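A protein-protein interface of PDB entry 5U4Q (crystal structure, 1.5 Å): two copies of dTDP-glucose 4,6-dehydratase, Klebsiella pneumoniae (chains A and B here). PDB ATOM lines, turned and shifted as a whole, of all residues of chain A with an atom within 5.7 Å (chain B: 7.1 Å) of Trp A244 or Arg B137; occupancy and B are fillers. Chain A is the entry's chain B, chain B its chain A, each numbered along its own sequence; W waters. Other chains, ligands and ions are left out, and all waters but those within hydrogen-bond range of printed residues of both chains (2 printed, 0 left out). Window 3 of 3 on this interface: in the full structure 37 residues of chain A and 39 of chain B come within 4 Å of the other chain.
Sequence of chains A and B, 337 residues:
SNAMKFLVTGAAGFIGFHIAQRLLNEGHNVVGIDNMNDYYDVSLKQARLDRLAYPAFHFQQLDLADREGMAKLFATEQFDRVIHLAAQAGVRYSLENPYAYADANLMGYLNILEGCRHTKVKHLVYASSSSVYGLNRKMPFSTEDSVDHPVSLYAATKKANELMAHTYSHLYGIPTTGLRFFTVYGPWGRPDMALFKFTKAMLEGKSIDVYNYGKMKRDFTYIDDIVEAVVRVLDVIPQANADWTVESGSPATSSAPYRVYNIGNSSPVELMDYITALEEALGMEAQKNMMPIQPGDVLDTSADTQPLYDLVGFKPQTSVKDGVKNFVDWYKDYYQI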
ATOM      1  N   HIS A 166       2.951  -9.470 -34.876  1.00  0.00           N
ATOM      2  CA  HIS A 166       3.748  -9.696 -33.657  1.00  0.00           C
ATOM      3  C   HIS A 166       2.912  -9.525 -32.401  1.00  0.00           C
ATOM      4  O   HIS A 166       2.955 -10.354 -31.464  1.00  0.00           O
ATOM      5  CB  HIS A 166       4.985  -8.780 -33.562  1.00  0.00           C
ATOM      6  CG  HIS A 166       5.829  -9.101 -32.377  1.00  0.00           C
ATOM      7  ND1 HIS A 166       5.656  -8.497 -31.157  1.00  0.00           N
ATOM      8  CD2 HIS A 166       6.752 -10.076 -32.187  1.00  0.00           C
ATOM      9  CE1 HIS A 166       6.463  -9.061 -30.269  1.00  0.00           C
ATOM     10  NE2 HIS A 166       7.147 -10.013 -30.873  1.00  0.00           N
ATOM     11  N   ASN A 241       9.328 -19.241 -27.950  1.00  0.00           N
ATOM     12  CA  ASN A 241      10.732 -19.452 -27.544  1.00  0.00           C
ATOM     13  C   ASN A 241      10.985 -18.555 -26.340  1.00  0.00           C
ATOM     14  O   ASN A 241      11.333 -17.395 -26.483  1.00  0.00           O
ATOM     15  CB  ASN A 241      11.710 -19.149 -28.698  1.00  0.00           C
ATOM     16  CG  ASN A 241      13.184 -19.309 -28.299  1.00  0.00           C
ATOM     17  OD1 ASN A 241      13.510 -19.822 -27.232  1.00  0.00           O
ATOM     18  ND2 ASN A 241      14.075 -18.859 -29.168  1.00  0.00           N
ATOM     19  N   ALA A 242      10.803 -19.119 -25.152  1.00  0.00           N
ATOM     20  CA  ALA A 242      10.971 -18.386 -23.890  1.00  0.00           C
ATOM     21  C   ALA A 242      12.359 -17.755 -23.648  1.00  0.00           C
ATOM     22  O   ALA A 242      12.466 -16.826 -22.852  1.00  0.00           O
ATOM     23  CB  ALA A 242      10.594 -19.281 -22.722  1.00  0.00           C
ATOM     24  N   ASP A 243      13.384 -18.231 -24.358  1.00  0.00           N
ATOM     25  CA  ASP A 243      14.762 -17.716 -24.215  1.00  0.00           C
ATOM     26  C   ASP A 243      15.103 -16.559 -25.152  1.00  0.00           C
ATOM     27  O   ASP A 243      16.159 -15.945 -25.015  1.00  0.00           O
ATOM     28  CB  ASP A 243      15.780 -18.842 -24.481  1.00  0.00           C
ATOM     29  CG  ASP A 243      15.672 -19.996 -23.486  1.00  0.00           C
ATOM     30  OD1 ASP A 243      15.091 -19.821 -22.393  1.00  0.00           O
ATOM     31  OD2 ASP A 243      16.193 -21.081 -23.805  1.00  0.00           O
ATOM     32  N   TRP A 244      14.235 -16.269 -26.119  1.00  0.00           N
ATOM     33  CA  TRP A 244      14.511 -15.212 -27.094  1.00  0.00           C
ATOM     34  C   TRP A 244      14.476 -13.823 -26.453  1.00  0.00           C
ATOM     35  O   TRP A 244      13.642 -13.547 -25.599  1.00  0.00           O
ATOM     36  CB  TRP A 244      13.490 -15.278 -28.238  1.00  0.00           C
ATOM     37  CG  TRP A 244      13.713 -14.318 -29.369  1.00  0.00           C
ATOM     38  CD1 TRP A 244      14.319 -14.583 -30.545  1.00  0.00           C
ATOM     39  CD2 TRP A 244      13.290 -12.944 -29.434  1.00  0.00           C
ATOM     40  NE1 TRP A 244      14.319 -13.474 -31.348  1.00  0.00           N
ATOM     41  CE2 TRP A 244      13.703 -12.447 -30.681  1.00  0.00           C
ATOM     42  CE3 TRP A 244      12.612 -12.093 -28.553  1.00  0.00           C
ATOM     43  CZ2 TRP A 244      13.458 -11.140 -31.080  1.00  0.00           C
ATOM     44  CZ3 TRP A 244      12.365 -10.794 -28.953  1.00  0.00           C
ATOM     45  CH2 TRP A 244      12.792 -10.330 -30.199  1.00  0.00           C
ATOM     46  N   THR A 245      15.413 -12.974 -26.863  1.00  0.00           N
ATOM     47  CA  THR A 245      15.452 -11.584 -26.411  1.00  0.00           C
ATOM     48  C   THR A 245      15.676 -10.720 -27.631  1.00  0.00           C
ATOM     49  O   THR A 245      16.235 -11.158 -28.630  1.00  0.00           O
ATOM     50  CB  THR A 245      16.602 -11.302 -25.402  1.00  0.00           C
ATOM     51  OG1 THR A 245      17.865 -11.418 -26.063  1.00  0.00           O
ATOM     52  CG2 THR A 245      16.553 -12.244 -24.218  1.00  0.00           C
ATOM     53  N   VAL A 246      15.234  -9.470 -27.550  1.00  0.00           N
ATOM     54  CA  VAL A 246      15.458  -8.522 -28.621  1.00  0.00           C
ATOM     55  C   VAL A 246      16.951  -8.308 -28.857  1.00  0.00           C
ATOM     56  O   VAL A 246      17.416  -8.231 -29.991  1.00  0.00           O
ATOM     57  CB  VAL A 246      14.805  -7.153 -28.263  1.00  0.00           C
ATOM     58  CG1 VAL A 246      15.250  -6.062 -29.228  1.00  0.00           C
ATOM     59  CG2 VAL A 246      13.281  -7.275 -28.231  1.00  0.00           C
ATOM     60  N   GLU A 247      17.694  -8.261 -27.760  1.00  0.00           N
ATOM     61  CA  GLU A 247      19.114  -7.940 -27.806  1.00  0.00           C
ATOM     62  C   GLU A 247      19.997  -8.988 -28.505  1.00  0.00           C
ATOM     63  O   GLU A 247      21.028  -8.633 -29.079  1.00  0.00           O
ATOM     64  CB  GLU A 247      19.605  -7.635 -26.391  1.00  0.00           C
ATOM     65  CG  GLU A 247      18.974  -6.372 -25.782  1.00  0.00           C
ATOM     66  CD  GLU A 247      17.495  -6.510 -25.387  1.00  0.00           C
ATOM     67  OE1 GLU A 247      17.044  -7.627 -25.024  1.00  0.00           O
ATOM     68  OE2 GLU A 247      16.769  -5.465 -25.408  1.00  0.00           O
ATOM     69  N   SER A 248      19.586 -10.257 -28.471  1.00  0.00           N
ATOM     70  CA  SER A 248      20.332 -11.329 -29.156  1.00  0.00           C
ATOM     71  C   SER A 248      19.537 -12.005 -30.289  1.00  0.00           C
ATOM     72  O   SER A 248      20.042 -12.932 -30.907  1.00  0.00           O
ATOM     73  CB  SER A 248      20.838 -12.374 -28.149  1.00  0.00           C
ATOM     74  OG  SER A 248      19.779 -13.102 -27.549  1.00  0.00           O
ATOM     75  N   GLY A 249      18.324 -11.512 -30.576  1.00  0.00           N
ATOM     76  CA  GLY A 249      17.461 -12.047 -31.646  1.00  0.00           C
ATOM     77  C   GLY A 249      17.339 -11.154 -32.877  1.00  0.00           C
ATOM     78  O   GLY A 249      18.276 -10.460 -33.223  1.00  0.00           O
ATOM     79  N   SER A 250      16.151 -11.140 -33.507  1.00  0.00           N
ATOM     80  CA  SER A 250      15.906 -10.439 -34.789  1.00  0.00           C
ATOM     81  C   SER A 250      14.523  -9.785 -34.971  1.00  0.00           C
ATOM     82  O   SER A 250      13.577 -10.137 -34.276  1.00  0.00           O
ATOM     83  CB  SER A 250      16.092 -11.464 -35.913  1.00  0.00           C
ATOM     84  OG  SER A 250      15.155 -11.302 -36.973  1.00  0.00           O
ATOM     85  N   PRO A 251      14.399  -8.843 -35.936  1.00  0.00           N
ATOM     86  CA  PRO A 251      13.094  -8.255 -36.265  1.00  0.00           C
ATOM     87  C   PRO A 251      12.136  -9.273 -36.947  1.00  0.00           C
ATOM     88  O   PRO A 251      10.963  -8.937 -37.259  1.00  0.00           O
ATOM     89  CB  PRO A 251      13.457  -7.128 -37.242  1.00  0.00           C
ATOM     90  CG  PRO A 251      14.911  -6.883 -37.064  1.00  0.00           C
ATOM     91  CD  PRO A 251      15.483  -8.214 -36.711  1.00  0.00           C
ATOM     92  N   THR A 253      12.092 -12.709 -35.717  1.00  0.00           N
ATOM     93  CA  THR A 253      11.873 -13.748 -34.735  1.00  0.00           C
ATOM     94  C   THR A 253      11.281 -13.105 -33.496  1.00  0.00           C
ATOM     95  O   THR A 253      11.173 -11.905 -33.424  1.00  0.00           O
ATOM     96  CB  THR A 253      13.224 -14.384 -34.333  1.00  0.00           C
ATOM     97  OG1 THR A 253      14.167 -13.342 -34.031  1.00  0.00           O
ATOM     98  CG2 THR A 253      13.762 -15.228 -35.468  1.00  0.00           C
ATOM     99  N   SER A 254      10.902 -13.917 -32.519  1.00  0.00           N
ATOM    100  CA  SER A 254      10.410 -13.438 -31.257  1.00  0.00           C
ATOM    101  C   SER A 254      10.343 -14.564 -30.266  1.00  0.00           C
ATOM    102  O   SER A 254      10.580 -15.739 -30.600  1.00  0.00           O
ATOM    103  CB  SER A 254       8.998 -12.797 -31.397  1.00  0.00           C
ATOM    104  OG  SER A 254       8.484 -12.347 -30.171  1.00  0.00           O
ATOM    105  N   SER A 255       9.997 -14.185 -29.047  1.00  0.00           N
ATOM    106  CA  SER A 255       9.667 -15.114 -28.002  1.00  0.00           C
ATOM    107  C   SER A 255       8.251 -15.607 -28.299  1.00  0.00           C
ATOM    108  O   SER A 255       7.848 -16.693 -27.884  1.00  0.00           O
ATOM    109  CB  SER A 255       9.755 -14.457 -26.612  1.00  0.00           C
ATOM    110  OG  SER A 255       9.157 -13.159 -26.596  1.00  0.00           O
ATOM    111  N   TYR B 133       8.662   0.385 -27.403  1.00  0.00           N
ATOM    112  CA  TYR B 133       9.865  -0.373 -26.961  1.00  0.00           C
ATOM    113  C   TYR B 133       9.547  -1.842 -26.747  1.00  0.00           C
ATOM    114  O   TYR B 133      10.442  -2.658 -26.767  1.00  0.00           O
ATOM    115  CB  TYR B 133      10.577   0.311 -25.765  1.00  0.00           C
ATOM    116  CG  TYR B 133      11.191   1.647 -26.207  1.00  0.00           C
ATOM    117  CD1 TYR B 133      12.252   1.671 -27.096  1.00  0.00           C
ATOM    118  CD2 TYR B 133      10.680   2.878 -25.762  1.00  0.00           C
ATOM    119  CE1 TYR B 133      12.804   2.836 -27.526  1.00  0.00           C
ATOM    120  CE2 TYR B 133      11.231   4.073 -26.189  1.00  0.00           C
ATOM    121  CZ  TYR B 133      12.283   4.057 -27.072  1.00  0.00           C
ATOM    122  OH  TYR B 133      12.844   5.209 -27.538  1.00  0.00           O
ATOM    123  N   GLY B 134       8.265  -2.169 -26.569  1.00  0.00           N
ATOM    124  CA  GLY B 134       7.812  -3.572 -26.545  1.00  0.00           C
ATOM    125  C   GLY B 134       8.623  -4.525 -25.689  1.00  0.00           C
ATOM    126  O   GLY B 134       8.764  -4.307 -24.509  1.00  0.00           O
ATOM    127  N   LEU B 135       9.144  -5.572 -26.319  1.00  0.00           N
ATOM    128  CA  LEU B 135       9.903  -6.617 -25.603  1.00  0.00           C
ATOM    129  C   LEU B 135      11.330  -6.210 -25.270  1.00  0.00           C
ATOM    130  O   LEU B 135      12.047  -6.991 -24.629  1.00  0.00           O
ATOM    131  CB  LEU B 135       9.922  -7.900 -26.432  1.00  0.00           C
ATOM    132  CG  LEU B 135       8.597  -8.672 -26.601  1.00  0.00           C
ATOM    133  CD1 LEU B 135       8.778  -9.799 -27.605  1.00  0.00           C
ATOM    134  CD2 LEU B 135       8.105  -9.197 -25.266  1.00  0.00           C
ATOM    135  N   ASN B 136      11.768  -5.024 -25.704  1.00  0.00           N
ATOM    136  CA  ASN B 136      13.136  -4.573 -25.419  1.00  0.00           C
ATOM    137  C   ASN B 136      13.447  -4.598 -23.924  1.00  0.00           C
ATOM    138  O   ASN B 136      12.596  -4.260 -23.098  1.00  0.00           O
ATOM    139  CB  ASN B 136      13.390  -3.132 -25.880  1.00  0.00           C
ATOM    140  CG  ASN B 136      13.336  -2.955 -27.386  1.00  0.00           C
ATOM    141  OD1 ASN B 136      12.804  -3.795 -28.127  1.00  0.00           O
ATOM    142  ND2 ASN B 136      13.849  -1.820 -27.844  1.00  0.00           N
ATOM    143  N   ARG B 137      14.676  -5.001 -23.591  1.00  0.00           N
ATOM    144  CA  ARG B 137      15.142  -5.058 -22.199  1.00  0.00           C
ATOM    145  C   ARG B 137      16.376  -4.194 -21.899  1.00  0.00           C
ATOM    146  O   ARG B 137      16.605  -3.849 -20.747  1.00  0.00           O
ATOM    147  CB  ARG B 137      15.395  -6.516 -21.787  1.00  0.00           C
ATOM    148  CG  ARG B 137      14.170  -7.171 -21.163  1.00  0.00           C
ATOM    149  CD  ARG B 137      14.250  -8.690 -21.135  1.00  0.00           C
ATOM    150  NE  ARG B 137      13.844  -9.259 -22.414  1.00  0.00           N
ATOM    151  CZ  ARG B 137      13.662 -10.554 -22.641  1.00  0.00           C
ATOM    152  NH1 ARG B 137      13.281 -10.955 -23.841  1.00  0.00           N
ATOM    153  NH2 ARG B 137      13.853 -11.443 -21.675  1.00  0.00           N
ATOM    154  N   LYS B 138      17.147  -3.835 -22.924  1.00  0.00           N
ATOM    155  CA  LYS B 138      18.350  -3.009 -22.725  1.00  0.00           C
ATOM    156  C   LYS B 138      17.957  -1.601 -22.285  1.00  0.00           C
ATOM    157  O   LYS B 138      17.188  -0.926 -22.985  1.00  0.00           O
ATOM    158  CB  LYS B 138      19.178  -2.932 -24.010  1.00  0.00           C
ATOM    159  CG  LYS B 138      20.462  -2.117 -23.861  1.00  0.00           C
ATOM    160  CD  LYS B 138      20.677  -1.104 -24.986  1.00  0.00           C
ATOM    161  CE  LYS B 138      19.494  -0.145 -25.077  1.00  0.00           C
ATOM    162  NZ  LYS B 138      19.750   1.193 -25.662  1.00  0.00           N
ATOM    163  N   MET B 139      18.462  -1.170 -21.125  1.00  0.00           N
ATOM    164  CA  MET B 139      18.193   0.173 -20.593  1.00  0.00           C
ATOM    165  C   MET B 139      19.426   1.036 -20.716  1.00  0.00           C
ATOM    166  O   MET B 139      20.543   0.518 -20.662  1.00  0.00           O
ATOM    167  CB  MET B 139      17.850   0.131 -19.115  1.00  0.00           C
ATOM    168  CG  MET B 139      16.650  -0.741 -18.812  1.00  0.00           C
ATOM    169  SD  MET B 139      15.069  -0.068 -19.775  1.00  0.00           S
ATOM    170  CE  MET B 139      13.895  -1.590 -19.322  1.00  0.00           C
ATOM    171  N   PRO B 140      19.270   2.351 -20.916  1.00  0.00           N
ATOM    172  CA  PRO B 140      17.977   3.029 -21.065  1.00  0.00           C
ATOM    173  C   PRO B 140      17.358   2.824 -22.441  1.00  0.00           C
ATOM    174  O   PRO B 140      18.064   2.565 -23.382  1.00  0.00           O
ATOM    175  CB  PRO B 140      18.368   4.499 -20.965  1.00  0.00           C
ATOM    176  CG  PRO B 140      19.711   4.543 -21.589  1.00  0.00           C
ATOM    177  CD  PRO B 140      20.391   3.289 -21.084  1.00  0.00           C
ATOM    178  N   PHE B 141      16.041   2.965 -22.546  1.00  0.00           N
ATOM    179  CA  PHE B 141      15.395   2.922 -23.848  1.00  0.00           C
ATOM    180  C   PHE B 141      15.852   4.132 -24.661  1.00  0.00           C
ATOM    181  O   PHE B 141      15.714   5.272 -24.207  1.00  0.00           O
ATOM    182  CB  PHE B 141      13.857   2.952 -23.721  1.00  0.00           C
ATOM    183  CG  PHE B 141      13.238   1.699 -23.156  1.00  0.00           C
ATOM    184  CD1 PHE B 141      13.727   0.423 -23.476  1.00  0.00           C
ATOM    185  CD2 PHE B 141      12.095   1.786 -22.376  1.00  0.00           C
ATOM    186  CE1 PHE B 141      13.116  -0.729 -22.964  1.00  0.00           C
ATOM    187  CE2 PHE B 141      11.472   0.648 -21.889  1.00  0.00           C
ATOM    188  CZ  PHE B 141      11.979  -0.613 -22.184  1.00  0.00           C
ATOM    189  N   HIS B 149       8.968  -5.141 -32.010  1.00  0.00           N
ATOM    190  CA  HIS B 149       8.298  -6.202 -31.247  1.00  0.00           C
ATOM    191  C   HIS B 149       7.315  -5.667 -30.247  1.00  0.00           C
ATOM    192  O   HIS B 149       7.459  -5.857 -29.048  1.00  0.00           O
ATOM    193  CB  HIS B 149       9.364  -7.056 -30.537  1.00  0.00           C
ATOM    194  CG  HIS B 149      10.284  -7.754 -31.469  1.00  0.00           C
ATOM    195  ND1 HIS B 149      11.519  -7.246 -31.807  1.00  0.00           N
ATOM    196  CD2 HIS B 149      10.161  -8.930 -32.132  1.00  0.00           C
ATOM    197  CE1 HIS B 149      12.108  -8.068 -32.658  1.00  0.00           C
ATOM    198  NE2 HIS B 149      11.302  -9.097 -32.873  1.00  0.00           N
HETATM  199  O   HOH W   1      11.297 -11.865 -25.171  1.00  0.00           O
HETATM  200  O   HOH W   2      14.335  -8.469 -24.954  1.00  0.00           O
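Water W1 lies within hydrogen-bond range of NH1 of Arg B137 (2.6 Å), OG of Ser A255 (2.9 Å) and O of Trp A244 (2.9 Å). Water W2 lies within hydrogen-bond range of the guanidinium group of Arg B137 (2.7 Å), the backbone carbonyl oxygen of Leu B135 (2.7 Å), the side-chain carboxylate of Glu A247 (2.8 Å) and the backbone NH of Val A246 (2.9 Å).
NH1 of Arg B137 sits at hydrogen-bond distance from O of Trp A244, at 3.2 Å. The side-chain carboxylate (OE2) of Glu A247 sits at hydrogen-bond distance from the backbone NH (N) of Lys B138, 3.0 Å away. OE2 of Glu A247 sits at hydrogen-bond distance from N of Arg B137, at 2.8 Å. O of Ser A250 lies within hydrogen-bond range of NE2 of His B149. A ring nitrogen (NE2) of His B149 is in hydrogen-bond range of the backbone carbonyl oxygen of Thr A253 (2.9 Å).
Printed residues of chain A that touch a printed residue of chain B: His A166, Trp A244, Thr A245, Val A246, Glu A247, Ser A250, Pro A251, Thr A253, Ser A254 and Ser A255. Of the 10 printed residues of chain B, 5 touch a printed residue of chain A. Printed residues of chain B that touch a printed residue of chain A: Leu B135, Asn B136, Arg B137, Lys B138 and His B149. Among the printed residues, no Asp or Glu carboxylate lies within 4 Å of a Lys or Arg side-chain nitrogen of the other chain.
Of the printed residues of chain B, Trp A244 touches Leu B135 (3.96 Å), Arg B137 (3.2 Å) and His B149 (3.3 Å). Printed residues of chain A within 4 Å of Arg B137: Trp A244, Thr A245 and Glu A247. Printed residues of chain B within 4 Å of Glu A247: Asn B136 (3.7 Å), Arg B137 (2.8 Å) and Lys B138 (3.0 Å). Of the printed residues of chain A, Asn B136 touches Val A246 and Glu A247. Of the printed residues of chain A, His B149 touches His A166 (3.4 Å), Trp A244 (3.3 Å), Val A246 (3.99 Å), Ser A250 (2.9 Å), Pro A251 (3.7 Å) and Thr A253 (2.9 Å). The nearest printed residue of chain B that does not touch Trp A244 is Asn B136 (6.6 Å). The nearest printed residue of chain A that does not touch Arg B137 is Val A246 (4.4 Å).
The backbone NH (N) of Ser A250 lies within hydrogen-bond range of the side-chain hydroxyl (OG1) of Thr A253 (3.0 Å). NZ of Lys B138 is in hydrogen-bond range of O of Pro B140, 3.2 Å away. The backbone carbonyl oxygen (O) of Ser A255 lies within hydrogen-bond range of the backbone NH (N) of Asn A241 (2.9 Å). OG1 of Thr A245 is in hydrogen-bond range of OG of Ser A248. N of Leu B135 sits at hydrogen-bond distance from O of His B149, at 3.2 Å. The side-chain amide oxygen (OD1) of Asn B136 lies close to the backbone carbonyl oxygen (O) of Tyr B133 (3.0 Å).
No position is printed for both chains.
Among the printed residues, merely in contact across the chains: Trp A244 with His B149, His A166 with His B149, Thr A245 with Arg B137, Val A246 with Asn B136, Ser A255 with Leu B135, His A166 with Leu B135, Ser A254 with Leu B135, Val A246 with Leu B135, Glu A247 with Asn B136, Pro A251 with His B149, Trp A244 with Leu B135 and Val A246 with His B149.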
